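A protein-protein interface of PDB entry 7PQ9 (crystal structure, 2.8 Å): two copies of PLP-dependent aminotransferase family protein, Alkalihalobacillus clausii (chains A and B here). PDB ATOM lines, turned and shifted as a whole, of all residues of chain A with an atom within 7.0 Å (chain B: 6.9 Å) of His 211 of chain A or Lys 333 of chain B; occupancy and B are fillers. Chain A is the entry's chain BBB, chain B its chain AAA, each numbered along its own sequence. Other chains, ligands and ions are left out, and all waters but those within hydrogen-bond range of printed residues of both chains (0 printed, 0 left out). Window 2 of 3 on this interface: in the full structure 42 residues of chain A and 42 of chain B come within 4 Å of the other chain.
The side-chain amino group (NZ) of Lys 333 of chain B is in hydrogen-bond range of a ring nitrogen (ND1) of His 211 of chain A (2.8 Å). NE2 of His 211 of chain A sits at hydrogen-bond distance from OH of Tyr 336 of chain B, at 2.6 Å. The side-chain hydroxyl (OH) of Tyr 337 of chain B lies within hydrogen-bond range of the side-chain amide nitrogen (NE2) of Gln 183 of chain A (3.0 Å).
NE2 of Gln 183 of chain A lies within hydrogen-bond range of OH of Tyr 212 of chain A. The backbone carbonyl oxygen (O) of Lys 207 of chain A sits at hydrogen-bond distance from the side-chain hydroxyl (OG) of Ser 210 of chain A.
Gln 183 of chain A touches Leu 187 of chain B (NE2 to CD1, 3.6 Å). Tyr 336 of chain B touches Lys 207 of chain A (OH to O, 3.5 Å). Leu 208 of chain A touches Tyr 336 of chain B. CD2 of Leu 208 of chain A touches OH of Tyr 337 of chain B, at 3.8 Å. Leu 187 of chain B touches His 211 of chain A (CD2 to O, 3.9 Å). Tyr 212 of chain A touches Leu 187 of chain B (OH to CD1, 3.95 Å). Tyr 212 of chain A touches Tyr 212 of chain B.
Printed residues of chain B within 4 Å of Gln 183 of chain A: Leu 187 (3.6 Å) and Tyr 337 (3.0 Å). Of the printed residues of chain B, Leu 208 of chain A touches Tyr 336 (3.8 Å) and Tyr 337 (3.8 Å). His 211 of chain A touches three residues of chain B. Asn 214 of chain A touches none of the printed residues of chain B. Of the printed residues of chain A, Leu 187 of chain B touches Gln 183, His 211 and Tyr 212. Printed residues of chain A within 4 Å of Tyr 212 of chain B: Tyr 212. Pro 213 of chain B touches none of the printed residues of chain A. Of chain A, only His 211 (2.8 Å) comes within 4 Å of Lys 333 of chain B. Printed residues of chain A within 4 Å of Tyr 337 of chain B: Gln 183 and Leu 208.
Hydrophobic or aromatic side chains of chain B within 4 Å of the printed part of chain A: Leu 187, Tyr 212, Tyr 336 and Tyr 337. Among the printed residues, no Asp or Glu carboxylate lies within 4 Å of a Lys or Arg side-chain nitrogen of the other chain.
Tyr 212 of chain B touches its own counterpart, Tyr 212 of chain A. Of the 10 pairs that touch across the chains among the printed residues, 1 has its exchanged pair printed and touching as well.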
ATOM      1  N   GLN A 183     -33.469 -10.510   6.912  1.00  0.00           N
ATOM      2  CA  GLN A 183     -32.920  -9.340   7.577  1.00  0.00           C
ATOM      3  C   GLN A 183     -34.017  -8.299   7.698  1.00  0.00           C
ATOM      4  O   GLN A 183     -34.156  -7.667   8.753  1.00  0.00           O
ATOM      5  CB  GLN A 183     -31.624  -8.831   6.929  1.00  0.00           C
ATOM      6  CG  GLN A 183     -30.433  -9.669   7.407  1.00  0.00           C
ATOM      7  CD  GLN A 183     -29.116  -9.475   6.702  1.00  0.00           C
ATOM      8  OE1 GLN A 183     -28.916  -9.957   5.578  1.00  0.00           O
ATOM      9  NE2 GLN A 183     -28.196  -8.840   7.414  1.00  0.00           N
ATOM     10  N   ARG A 206     -29.578 -19.035  12.347  1.00  0.00           N
ATOM     11  CA  ARG A 206     -28.810 -18.808  13.555  1.00  0.00           C
ATOM     12  C   ARG A 206     -27.678 -17.810  13.269  1.00  0.00           C
ATOM     13  O   ARG A 206     -27.449 -16.866  14.030  1.00  0.00           O
ATOM     14  CB  ARG A 206     -28.266 -20.153  14.033  1.00  0.00           C
ATOM     15  CG  ARG A 206     -27.312 -19.971  15.197  1.00  0.00           C
ATOM     16  CD  ARG A 206     -26.643 -21.251  15.647  1.00  0.00           C
ATOM     17  NE  ARG A 206     -25.848 -21.890  14.597  1.00  0.00           N
ATOM     18  CZ  ARG A 206     -24.653 -21.464  14.183  1.00  0.00           C
ATOM     19  NH1 ARG A 206     -23.991 -22.134  13.255  1.00  0.00           N
ATOM     20  NH2 ARG A 206     -24.136 -20.358  14.670  1.00  0.00           N
ATOM     21  N   LYS A 207     -26.984 -18.033  12.148  1.00  0.00           N
ATOM     22  CA  LYS A 207     -25.857 -17.214  11.763  1.00  0.00           C
ATOM     23  C   LYS A 207     -26.279 -15.751  11.624  1.00  0.00           C
ATOM     24  O   LYS A 207     -25.674 -14.886  12.244  1.00  0.00           O
ATOM     25  CB  LYS A 207     -25.137 -17.799  10.546  1.00  0.00           C
ATOM     26  CG  LYS A 207     -24.262 -19.017  10.843  1.00  0.00           C
ATOM     27  CD  LYS A 207     -23.724 -19.701   9.610  1.00  0.00           C
ATOM     28  CE  LYS A 207     -22.779 -20.838   9.927  1.00  0.00           C
ATOM     29  NZ  LYS A 207     -22.302 -21.492   8.697  1.00  0.00           N
ATOM     30  N   LEU A 208     -27.331 -15.477  10.847  1.00  0.00           N
ATOM     31  CA  LEU A 208     -27.832 -14.111  10.692  1.00  0.00           C
ATOM     32  C   LEU A 208     -28.173 -13.497  12.050  1.00  0.00           C
ATOM     33  O   LEU A 208     -27.916 -12.321  12.282  1.00  0.00           O
ATOM     34  CB  LEU A 208     -29.065 -14.096   9.802  1.00  0.00           C
ATOM     35  CG  LEU A 208     -28.750 -14.272   8.326  1.00  0.00           C
ATOM     36  CD1 LEU A 208     -30.020 -14.544   7.544  1.00  0.00           C
ATOM     37  CD2 LEU A 208     -28.085 -13.019   7.803  1.00  0.00           C
ATOM     38  N   LEU A 209     -28.758 -14.302  12.944  1.00  0.00           N
ATOM     39  CA  LEU A 209     -29.270 -13.747  14.178  1.00  0.00           C
ATOM     40  C   LEU A 209     -28.129 -13.280  15.073  1.00  0.00           C
ATOM     41  O   LEU A 209     -28.349 -12.436  15.954  1.00  0.00           O
ATOM     42  CB  LEU A 209     -30.140 -14.783  14.885  1.00  0.00           C
ATOM     43  CG  LEU A 209     -31.587 -14.821  14.447  1.00  0.00           C
ATOM     44  CD1 LEU A 209     -32.222 -16.048  15.090  1.00  0.00           C
ATOM     45  CD2 LEU A 209     -32.300 -13.532  14.845  1.00  0.00           C
ATOM     46  N   SER A 210     -26.923 -13.814  14.831  1.00  0.00           N
ATOM     47  CA  SER A 210     -25.765 -13.390  15.601  1.00  0.00           C
ATOM     48  C   SER A 210     -25.477 -11.892  15.442  1.00  0.00           C
ATOM     49  O   SER A 210     -24.879 -11.303  16.338  1.00  0.00           O
ATOM     50  CB  SER A 210     -24.557 -14.212  15.306  1.00  0.00           C
ATOM     51  OG  SER A 210     -23.992 -13.797  14.075  1.00  0.00           O
ATOM     52  N   HIS A 211     -25.940 -11.258  14.358  1.00  0.00           N
ATOM     53  CA  HIS A 211     -25.669  -9.846  14.132  1.00  0.00           C
ATOM     54  C   HIS A 211     -26.788  -8.946  14.640  1.00  0.00           C
ATOM     55  O   HIS A 211     -26.670  -7.728  14.564  1.00  0.00           O
ATOM     56  CB  HIS A 211     -25.381  -9.550  12.650  1.00  0.00           C
ATOM     57  CG  HIS A 211     -24.419 -10.511  12.045  1.00  0.00           C
ATOM     58  ND1 HIS A 211     -23.135 -10.692  12.555  1.00  0.00           N
ATOM     59  CD2 HIS A 211     -24.541 -11.350  10.994  1.00  0.00           C
ATOM     60  CE1 HIS A 211     -22.522 -11.627  11.854  1.00  0.00           C
ATOM     61  NE2 HIS A 211     -23.364 -12.041  10.893  1.00  0.00           N
ATOM     62  N   TYR A 212     -27.897  -9.544  15.088  1.00  0.00           N
ATOM     63  CA  TYR A 212     -29.073  -8.758  15.443  1.00  0.00           C
ATOM     64  C   TYR A 212     -29.287  -8.878  16.949  1.00  0.00           C
ATOM     65  O   TYR A 212     -28.858  -9.862  17.570  1.00  0.00           O
ATOM     66  CB  TYR A 212     -30.278  -9.169  14.598  1.00  0.00           C
ATOM     67  CG  TYR A 212     -30.176  -8.710  13.162  1.00  0.00           C
ATOM     68  CD1 TYR A 212     -29.533  -9.501  12.207  1.00  0.00           C
ATOM     69  CD2 TYR A 212     -30.637  -7.458  12.776  1.00  0.00           C
ATOM     70  CE1 TYR A 212     -29.365  -9.059  10.897  1.00  0.00           C
ATOM     71  CE2 TYR A 212     -30.437  -6.997  11.481  1.00  0.00           C
ATOM     72  CZ  TYR A 212     -29.815  -7.804  10.535  1.00  0.00           C
ATOM     73  OH  TYR A 212     -29.635  -7.353   9.261  1.00  0.00           O
ATOM     74  N   PRO A 213     -29.923  -7.867  17.577  1.00  0.00           N
ATOM     75  CA  PRO A 213     -30.198  -7.880  19.018  1.00  0.00           C
ATOM     76  C   PRO A 213     -30.881  -9.140  19.531  1.00  0.00           C
ATOM     77  O   PRO A 213     -30.650  -9.558  20.662  1.00  0.00           O
ATOM     78  CB  PRO A 213     -31.189  -6.723  19.196  1.00  0.00           C
ATOM     79  CG  PRO A 213     -30.899  -5.776  18.032  1.00  0.00           C
ATOM     80  CD  PRO A 213     -30.434  -6.662  16.898  1.00  0.00           C
ATOM     81  N   ASN A 214     -31.709  -9.739  18.669  1.00  0.00           N
ATOM     82  CA  ASN A 214     -32.626 -10.840  18.937  1.00  0.00           C
ATOM     83  C   ASN A 214     -31.879 -12.107  19.381  1.00  0.00           C
ATOM     84  O   ASN A 214     -30.845 -12.440  18.802  1.00  0.00           O
ATOM     85  CB  ASN A 214     -33.439 -11.105  17.668  1.00  0.00           C
ATOM     86  CG  ASN A 214     -34.221  -9.868  17.296  1.00  0.00           C
ATOM     87  OD1 ASN A 214     -33.698  -8.979  16.636  1.00  0.00           O
ATOM     88  ND2 ASN A 214     -35.479  -9.801  17.705  1.00  0.00           N
ATOM     89  N   HIS B 145     -19.691 -15.261  -2.706  1.00  0.00           N
ATOM     90  CA  HIS B 145     -20.567 -14.277  -2.076  1.00  0.00           C
ATOM     91  C   HIS B 145     -20.189 -12.824  -2.347  1.00  0.00           C
ATOM     92  O   HIS B 145     -21.040 -11.973  -2.584  1.00  0.00           O
ATOM     93  CB  HIS B 145     -20.784 -14.596  -0.609  1.00  0.00           C
ATOM     94  CG  HIS B 145     -19.822 -13.995   0.343  1.00  0.00           C
ATOM     95  ND1 HIS B 145     -18.768 -14.740   0.830  1.00  0.00           N
ATOM     96  CD2 HIS B 145     -19.791 -12.787   0.965  1.00  0.00           C
ATOM     97  CE1 HIS B 145     -18.087 -14.034   1.716  1.00  0.00           C
ATOM     98  NE2 HIS B 145     -18.684 -12.821   1.791  1.00  0.00           N
ATOM     99  N   GLN B 184     -24.615  -3.928   5.400  1.00  0.00           N
ATOM    100  CA  GLN B 184     -23.591  -4.870   5.800  1.00  0.00           C
ATOM    101  C   GLN B 184     -22.486  -4.122   6.533  1.00  0.00           C
ATOM    102  O   GLN B 184     -21.957  -4.564   7.555  1.00  0.00           O
ATOM    103  CB  GLN B 184     -23.149  -5.666   4.601  1.00  0.00           C
ATOM    104  CG  GLN B 184     -24.090  -6.833   4.354  1.00  0.00           C
ATOM    105  CD  GLN B 184     -23.779  -7.423   3.009  1.00  0.00           C
ATOM    106  OE1 GLN B 184     -22.724  -7.213   2.434  1.00  0.00           O
ATOM    107  NE2 GLN B 184     -24.744  -8.130   2.467  1.00  0.00           N
ATOM    108  N   LEU B 187     -23.404  -3.410  10.222  1.00  0.00           N
ATOM    109  CA  LEU B 187     -23.223  -4.619  11.007  1.00  0.00           C
ATOM    110  C   LEU B 187     -21.742  -4.861  11.265  1.00  0.00           C
ATOM    111  O   LEU B 187     -21.381  -5.290  12.353  1.00  0.00           O
ATOM    112  CB  LEU B 187     -23.788  -5.817  10.243  1.00  0.00           C
ATOM    113  CG  LEU B 187     -25.290  -5.834   9.998  1.00  0.00           C
ATOM    114  CD1 LEU B 187     -25.687  -7.176   9.379  1.00  0.00           C
ATOM    115  CD2 LEU B 187     -26.019  -5.623  11.301  1.00  0.00           C
ATOM    116  N   LEU B 188     -20.915  -4.621  10.232  1.00  0.00           N
ATOM    117  CA  LEU B 188     -19.497  -4.929  10.270  1.00  0.00           C
ATOM    118  C   LEU B 188     -18.772  -4.045  11.278  1.00  0.00           C
ATOM    119  O   LEU B 188     -18.051  -4.585  12.111  1.00  0.00           O
ATOM    120  CB  LEU B 188     -18.914  -4.715   8.871  1.00  0.00           C
ATOM    121  CG  LEU B 188     -17.436  -5.047   8.724  1.00  0.00           C
ATOM    122  CD1 LEU B 188     -17.203  -6.518   8.922  1.00  0.00           C
ATOM    123  CD2 LEU B 188     -16.933  -4.591   7.375  1.00  0.00           C
ATOM    124  N   LEU B 189     -18.965  -2.721  11.196  1.00  0.00           N
ATOM    125  CA  LEU B 189     -18.249  -1.767  12.045  1.00  0.00           C
ATOM    126  C   LEU B 189     -18.739  -1.743  13.498  1.00  0.00           C
ATOM    127  O   LEU B 189     -18.134  -1.052  14.315  1.00  0.00           O
ATOM    128  CB  LEU B 189     -18.359  -0.341  11.458  1.00  0.00           C
ATOM    129  CG  LEU B 189     -17.796  -0.184  10.069  1.00  0.00           C
ATOM    130  CD1 LEU B 189     -17.872   1.279   9.620  1.00  0.00           C
ATOM    131  CD2 LEU B 189     -16.350  -0.632  10.095  1.00  0.00           C
ATOM    132  N   GLY B 190     -19.930  -2.345  13.747  1.00  0.00           N
ATOM    133  CA  GLY B 190     -20.429  -2.472  15.098  1.00  0.00           C
ATOM    134  C   GLY B 190     -21.401  -1.381  15.521  1.00  0.00           C
ATOM    135  O   GLY B 190     -21.486  -0.298  14.911  1.00  0.00           O
ATOM    136  N   TYR B 212     -30.980   0.755  12.797  1.00  0.00           N
ATOM    137  CA  TYR B 212     -29.811   0.156  13.430  1.00  0.00           C
ATOM    138  C   TYR B 212     -29.532   0.866  14.745  1.00  0.00           C
ATOM    139  O   TYR B 212     -29.921   2.023  14.916  1.00  0.00           O
ATOM    140  CB  TYR B 212     -28.630   0.161  12.443  1.00  0.00           C
ATOM    141  CG  TYR B 212     -28.804  -0.823  11.307  1.00  0.00           C
ATOM    142  CD1 TYR B 212     -28.445  -2.164  11.429  1.00  0.00           C
ATOM    143  CD2 TYR B 212     -29.508  -0.422  10.167  1.00  0.00           C
ATOM    144  CE1 TYR B 212     -28.772  -3.079  10.440  1.00  0.00           C
ATOM    145  CE2 TYR B 212     -29.813  -1.329   9.160  1.00  0.00           C
ATOM    146  CZ  TYR B 212     -29.421  -2.650   9.283  1.00  0.00           C
ATOM    147  OH  TYR B 212     -29.711  -3.527   8.280  1.00  0.00           O
ATOM    148  N   PRO B 213     -28.869   0.191  15.699  1.00  0.00           N
ATOM    149  CA  PRO B 213     -28.522   0.792  16.997  1.00  0.00           C
ATOM    150  C   PRO B 213     -27.795   2.128  16.908  1.00  0.00           C
ATOM    151  O   PRO B 213     -27.955   2.973  17.777  1.00  0.00           O
ATOM    152  CB  PRO B 213     -27.543  -0.219  17.618  1.00  0.00           C
ATOM    153  CG  PRO B 213     -27.896  -1.541  16.973  1.00  0.00           C
ATOM    154  CD  PRO B 213     -28.384  -1.196  15.570  1.00  0.00           C
ATOM    155  N   HIS B 328     -10.875  -8.147   5.335  1.00  0.00           N
ATOM    156  CA  HIS B 328     -10.546  -9.472   5.843  1.00  0.00           C
ATOM    157  C   HIS B 328     -11.595  -9.853   6.864  1.00  0.00           C
ATOM    158  O   HIS B 328     -12.069 -10.985   6.879  1.00  0.00           O
ATOM    159  CB  HIS B 328      -9.053  -9.635   6.228  1.00  0.00           C
ATOM    160  CG  HIS B 328      -8.179  -9.714   5.014  1.00  0.00           C
ATOM    161  ND1 HIS B 328      -7.216  -8.753   4.720  1.00  0.00           N
ATOM    162  CD2 HIS B 328      -8.181 -10.575   3.964  1.00  0.00           C
ATOM    163  CE1 HIS B 328      -6.644  -9.040   3.565  1.00  0.00           C
ATOM    164  NE2 HIS B 328      -7.233 -10.149   3.069  1.00  0.00           N
ATOM    165  N   LEU B 329     -11.997  -8.851   7.644  1.00  0.00           N
ATOM    166  CA  LEU B 329     -13.022  -9.006   8.654  1.00  0.00           C
ATOM    167  C   LEU B 329     -14.368  -9.348   8.010  1.00  0.00           C
ATOM    168  O   LEU B 329     -15.056 -10.280   8.421  1.00  0.00           O
ATOM    169  CB  LEU B 329     -13.071  -7.725   9.485  1.00  0.00           C
ATOM    170  CG  LEU B 329     -14.078  -7.807  10.623  1.00  0.00           C
ATOM    171  CD1 LEU B 329     -13.897  -9.097  11.426  1.00  0.00           C
ATOM    172  CD2 LEU B 329     -13.998  -6.585  11.523  1.00  0.00           C
ATOM    173  N   TYR B 330     -14.722  -8.603   6.963  1.00  0.00           N
ATOM    174  CA  TYR B 330     -15.899  -8.894   6.151  1.00  0.00           C
ATOM    175  C   TYR B 330     -15.884 -10.351   5.681  1.00  0.00           C
ATOM    176  O   TYR B 330     -16.829 -11.067   5.908  1.00  0.00           O
ATOM    177  CB  TYR B 330     -16.048  -7.884   5.015  1.00  0.00           C
ATOM    178  CG  TYR B 330     -17.268  -8.080   4.147  1.00  0.00           C
ATOM    179  CD1 TYR B 330     -17.393  -9.179   3.313  1.00  0.00           C
ATOM    180  CD2 TYR B 330     -18.304  -7.156   4.147  1.00  0.00           C
ATOM    181  CE1 TYR B 330     -18.516  -9.362   2.525  1.00  0.00           C
ATOM    182  CE2 TYR B 330     -19.440  -7.324   3.365  1.00  0.00           C
ATOM    183  CZ  TYR B 330     -19.543  -8.443   2.559  1.00  0.00           C
ATOM    184  OH  TYR B 330     -20.642  -8.685   1.781  1.00  0.00           O
ATOM    185  N   LYS B 331     -14.817 -10.809   5.032  1.00  0.00           N
ATOM    186  CA  LYS B 331     -14.794 -12.158   4.480  1.00  0.00           C
ATOM    187  C   LYS B 331     -15.002 -13.197   5.576  1.00  0.00           C
ATOM    188  O   LYS B 331     -15.450 -14.292   5.265  1.00  0.00           O
ATOM    189  CB  LYS B 331     -13.543 -12.414   3.627  1.00  0.00           C
ATOM    190  CG  LYS B 331     -13.479 -11.612   2.307  1.00  0.00           C
ATOM    191  CD  LYS B 331     -12.250 -11.851   1.434  1.00  0.00           C
ATOM    192  CE  LYS B 331     -12.186 -13.268   0.903  1.00  0.00           C
ATOM    193  NZ  LYS B 331     -10.846 -13.632   0.398  1.00  0.00           N
ATOM    194  N   ASN B 332     -14.718 -12.862   6.841  1.00  0.00           N
ATOM    195  CA  ASN B 332     -14.854 -13.822   7.936  1.00  0.00           C
ATOM    196  C   ASN B 332     -16.266 -13.785   8.509  1.00  0.00           C
ATOM    197  O   ASN B 332     -16.909 -14.836   8.650  1.00  0.00           O
ATOM    198  CB  ASN B 332     -13.918 -13.549   9.118  1.00  0.00           C
ATOM    199  CG  ASN B 332     -12.492 -13.971   8.896  1.00  0.00           C
ATOM    200  OD1 ASN B 332     -12.219 -14.833   8.059  1.00  0.00           O
ATOM    201  ND2 ASN B 332     -11.595 -13.362   9.654  1.00  0.00           N
ATOM    202  N   LYS B 333     -16.705 -12.558   8.837  1.00  0.00           N
ATOM    203  CA  LYS B 333     -17.978 -12.275   9.476  1.00  0.00           C
ATOM    204  C   LYS B 333     -19.132 -12.781   8.610  1.00  0.00           C
ATOM    205  O   LYS B 333     -20.067 -13.374   9.125  1.00  0.00           O
ATOM    206  CB  LYS B 333     -18.100 -10.782   9.790  1.00  0.00           C
ATOM    207  CG  LYS B 333     -19.329 -10.388  10.588  1.00  0.00           C
ATOM    208  CD  LYS B 333     -19.373  -8.930  11.051  1.00  0.00           C
ATOM    209  CE  LYS B 333     -20.590  -8.583  11.891  1.00  0.00           C
ATOM    210  NZ  LYS B 333     -20.729  -9.315  13.178  1.00  0.00           N
ATOM    211  N   PHE B 334     -19.045 -12.564   7.302  1.00  0.00           N
ATOM    212  CA  PHE B 334     -20.135 -12.844   6.385  1.00  0.00           C
ATOM    213  C   PHE B 334     -19.809 -14.016   5.464  1.00  0.00           C
ATOM    214  O   PHE B 334     -20.315 -14.087   4.317  1.00  0.00           O
ATOM    215  CB  PHE B 334     -20.473 -11.614   5.537  1.00  0.00           C
ATOM    216  CG  PHE B 334     -20.817 -10.380   6.340  1.00  0.00           C
ATOM    217  CD1 PHE B 334     -21.758 -10.408   7.349  1.00  0.00           C
ATOM    218  CD2 PHE B 334     -20.219  -9.175   6.077  1.00  0.00           C
ATOM    219  CE1 PHE B 334     -22.090  -9.277   8.066  1.00  0.00           C
ATOM    220  CE2 PHE B 334     -20.538  -8.037   6.789  1.00  0.00           C
ATOM    221  CZ  PHE B 334     -21.473  -8.084   7.794  1.00  0.00           C
ATOM    222  N   SER B 335     -19.052 -14.992   6.006  1.00  0.00           N
ATOM    223  CA  SER B 335     -18.578 -16.102   5.188  1.00  0.00           C
ATOM    224  C   SER B 335     -19.734 -16.930   4.627  1.00  0.00           C
ATOM    225  O   SER B 335     -19.585 -17.590   3.608  1.00  0.00           O
ATOM    226  CB  SER B 335     -17.622 -16.977   5.962  1.00  0.00           C
ATOM    227  OG  SER B 335     -18.120 -17.293   7.260  1.00  0.00           O
ATOM    228  N   TYR B 336     -20.891 -16.901   5.301  1.00  0.00           N
ATOM    229  CA  TYR B 336     -21.975 -17.831   5.044  1.00  0.00           C
ATOM    230  C   TYR B 336     -23.033 -17.196   4.148  1.00  0.00           C
ATOM    231  O   TYR B 336     -23.970 -17.883   3.752  1.00  0.00           O
ATOM    232  CB  TYR B 336     -22.621 -18.269   6.358  1.00  0.00           C
ATOM    233  CG  TYR B 336     -23.085 -17.077   7.147  1.00  0.00           C
ATOM    234  CD1 TYR B 336     -24.296 -16.461   6.857  1.00  0.00           C
ATOM    235  CD2 TYR B 336     -22.295 -16.526   8.146  1.00  0.00           C
ATOM    236  CE1 TYR B 336     -24.713 -15.329   7.540  1.00  0.00           C
ATOM    237  CE2 TYR B 336     -22.729 -15.425   8.879  1.00  0.00           C
ATOM    238  CZ  TYR B 336     -23.925 -14.804   8.547  1.00  0.00           C
ATOM    239  OH  TYR B 336     -24.360 -13.697   9.214  1.00  0.00           O
ATOM    240  N   TYR B 337     -22.914 -15.895   3.874  1.00  0.00           N
ATOM    241  CA  TYR B 337     -23.819 -15.201   2.966  1.00  0.00           C
ATOM    242  C   TYR B 337     -23.666 -15.694   1.530  1.00  0.00           C
ATOM    243  O   TYR B 337     -22.763 -16.443   1.192  1.00  0.00           O
ATOM    244  CB  TYR B 337     -23.515 -13.709   2.885  1.00  0.00           C
ATOM    245  CG  TYR B 337     -24.099 -12.832   3.959  1.00  0.00           C
ATOM    246  CD1 TYR B 337     -24.052 -13.199   5.294  1.00  0.00           C
ATOM    247  CD2 TYR B 337     -24.736 -11.639   3.640  1.00  0.00           C
ATOM    248  CE1 TYR B 337     -24.544 -12.373   6.291  1.00  0.00           C
ATOM    249  CE2 TYR B 337     -25.230 -10.803   4.636  1.00  0.00           C
ATOM    250  CZ  TYR B 337     -25.083 -11.140   5.968  1.00  0.00           C
ATOM    251  OH  TYR B 337     -25.571 -10.306   6.935  1.00  0.00           O
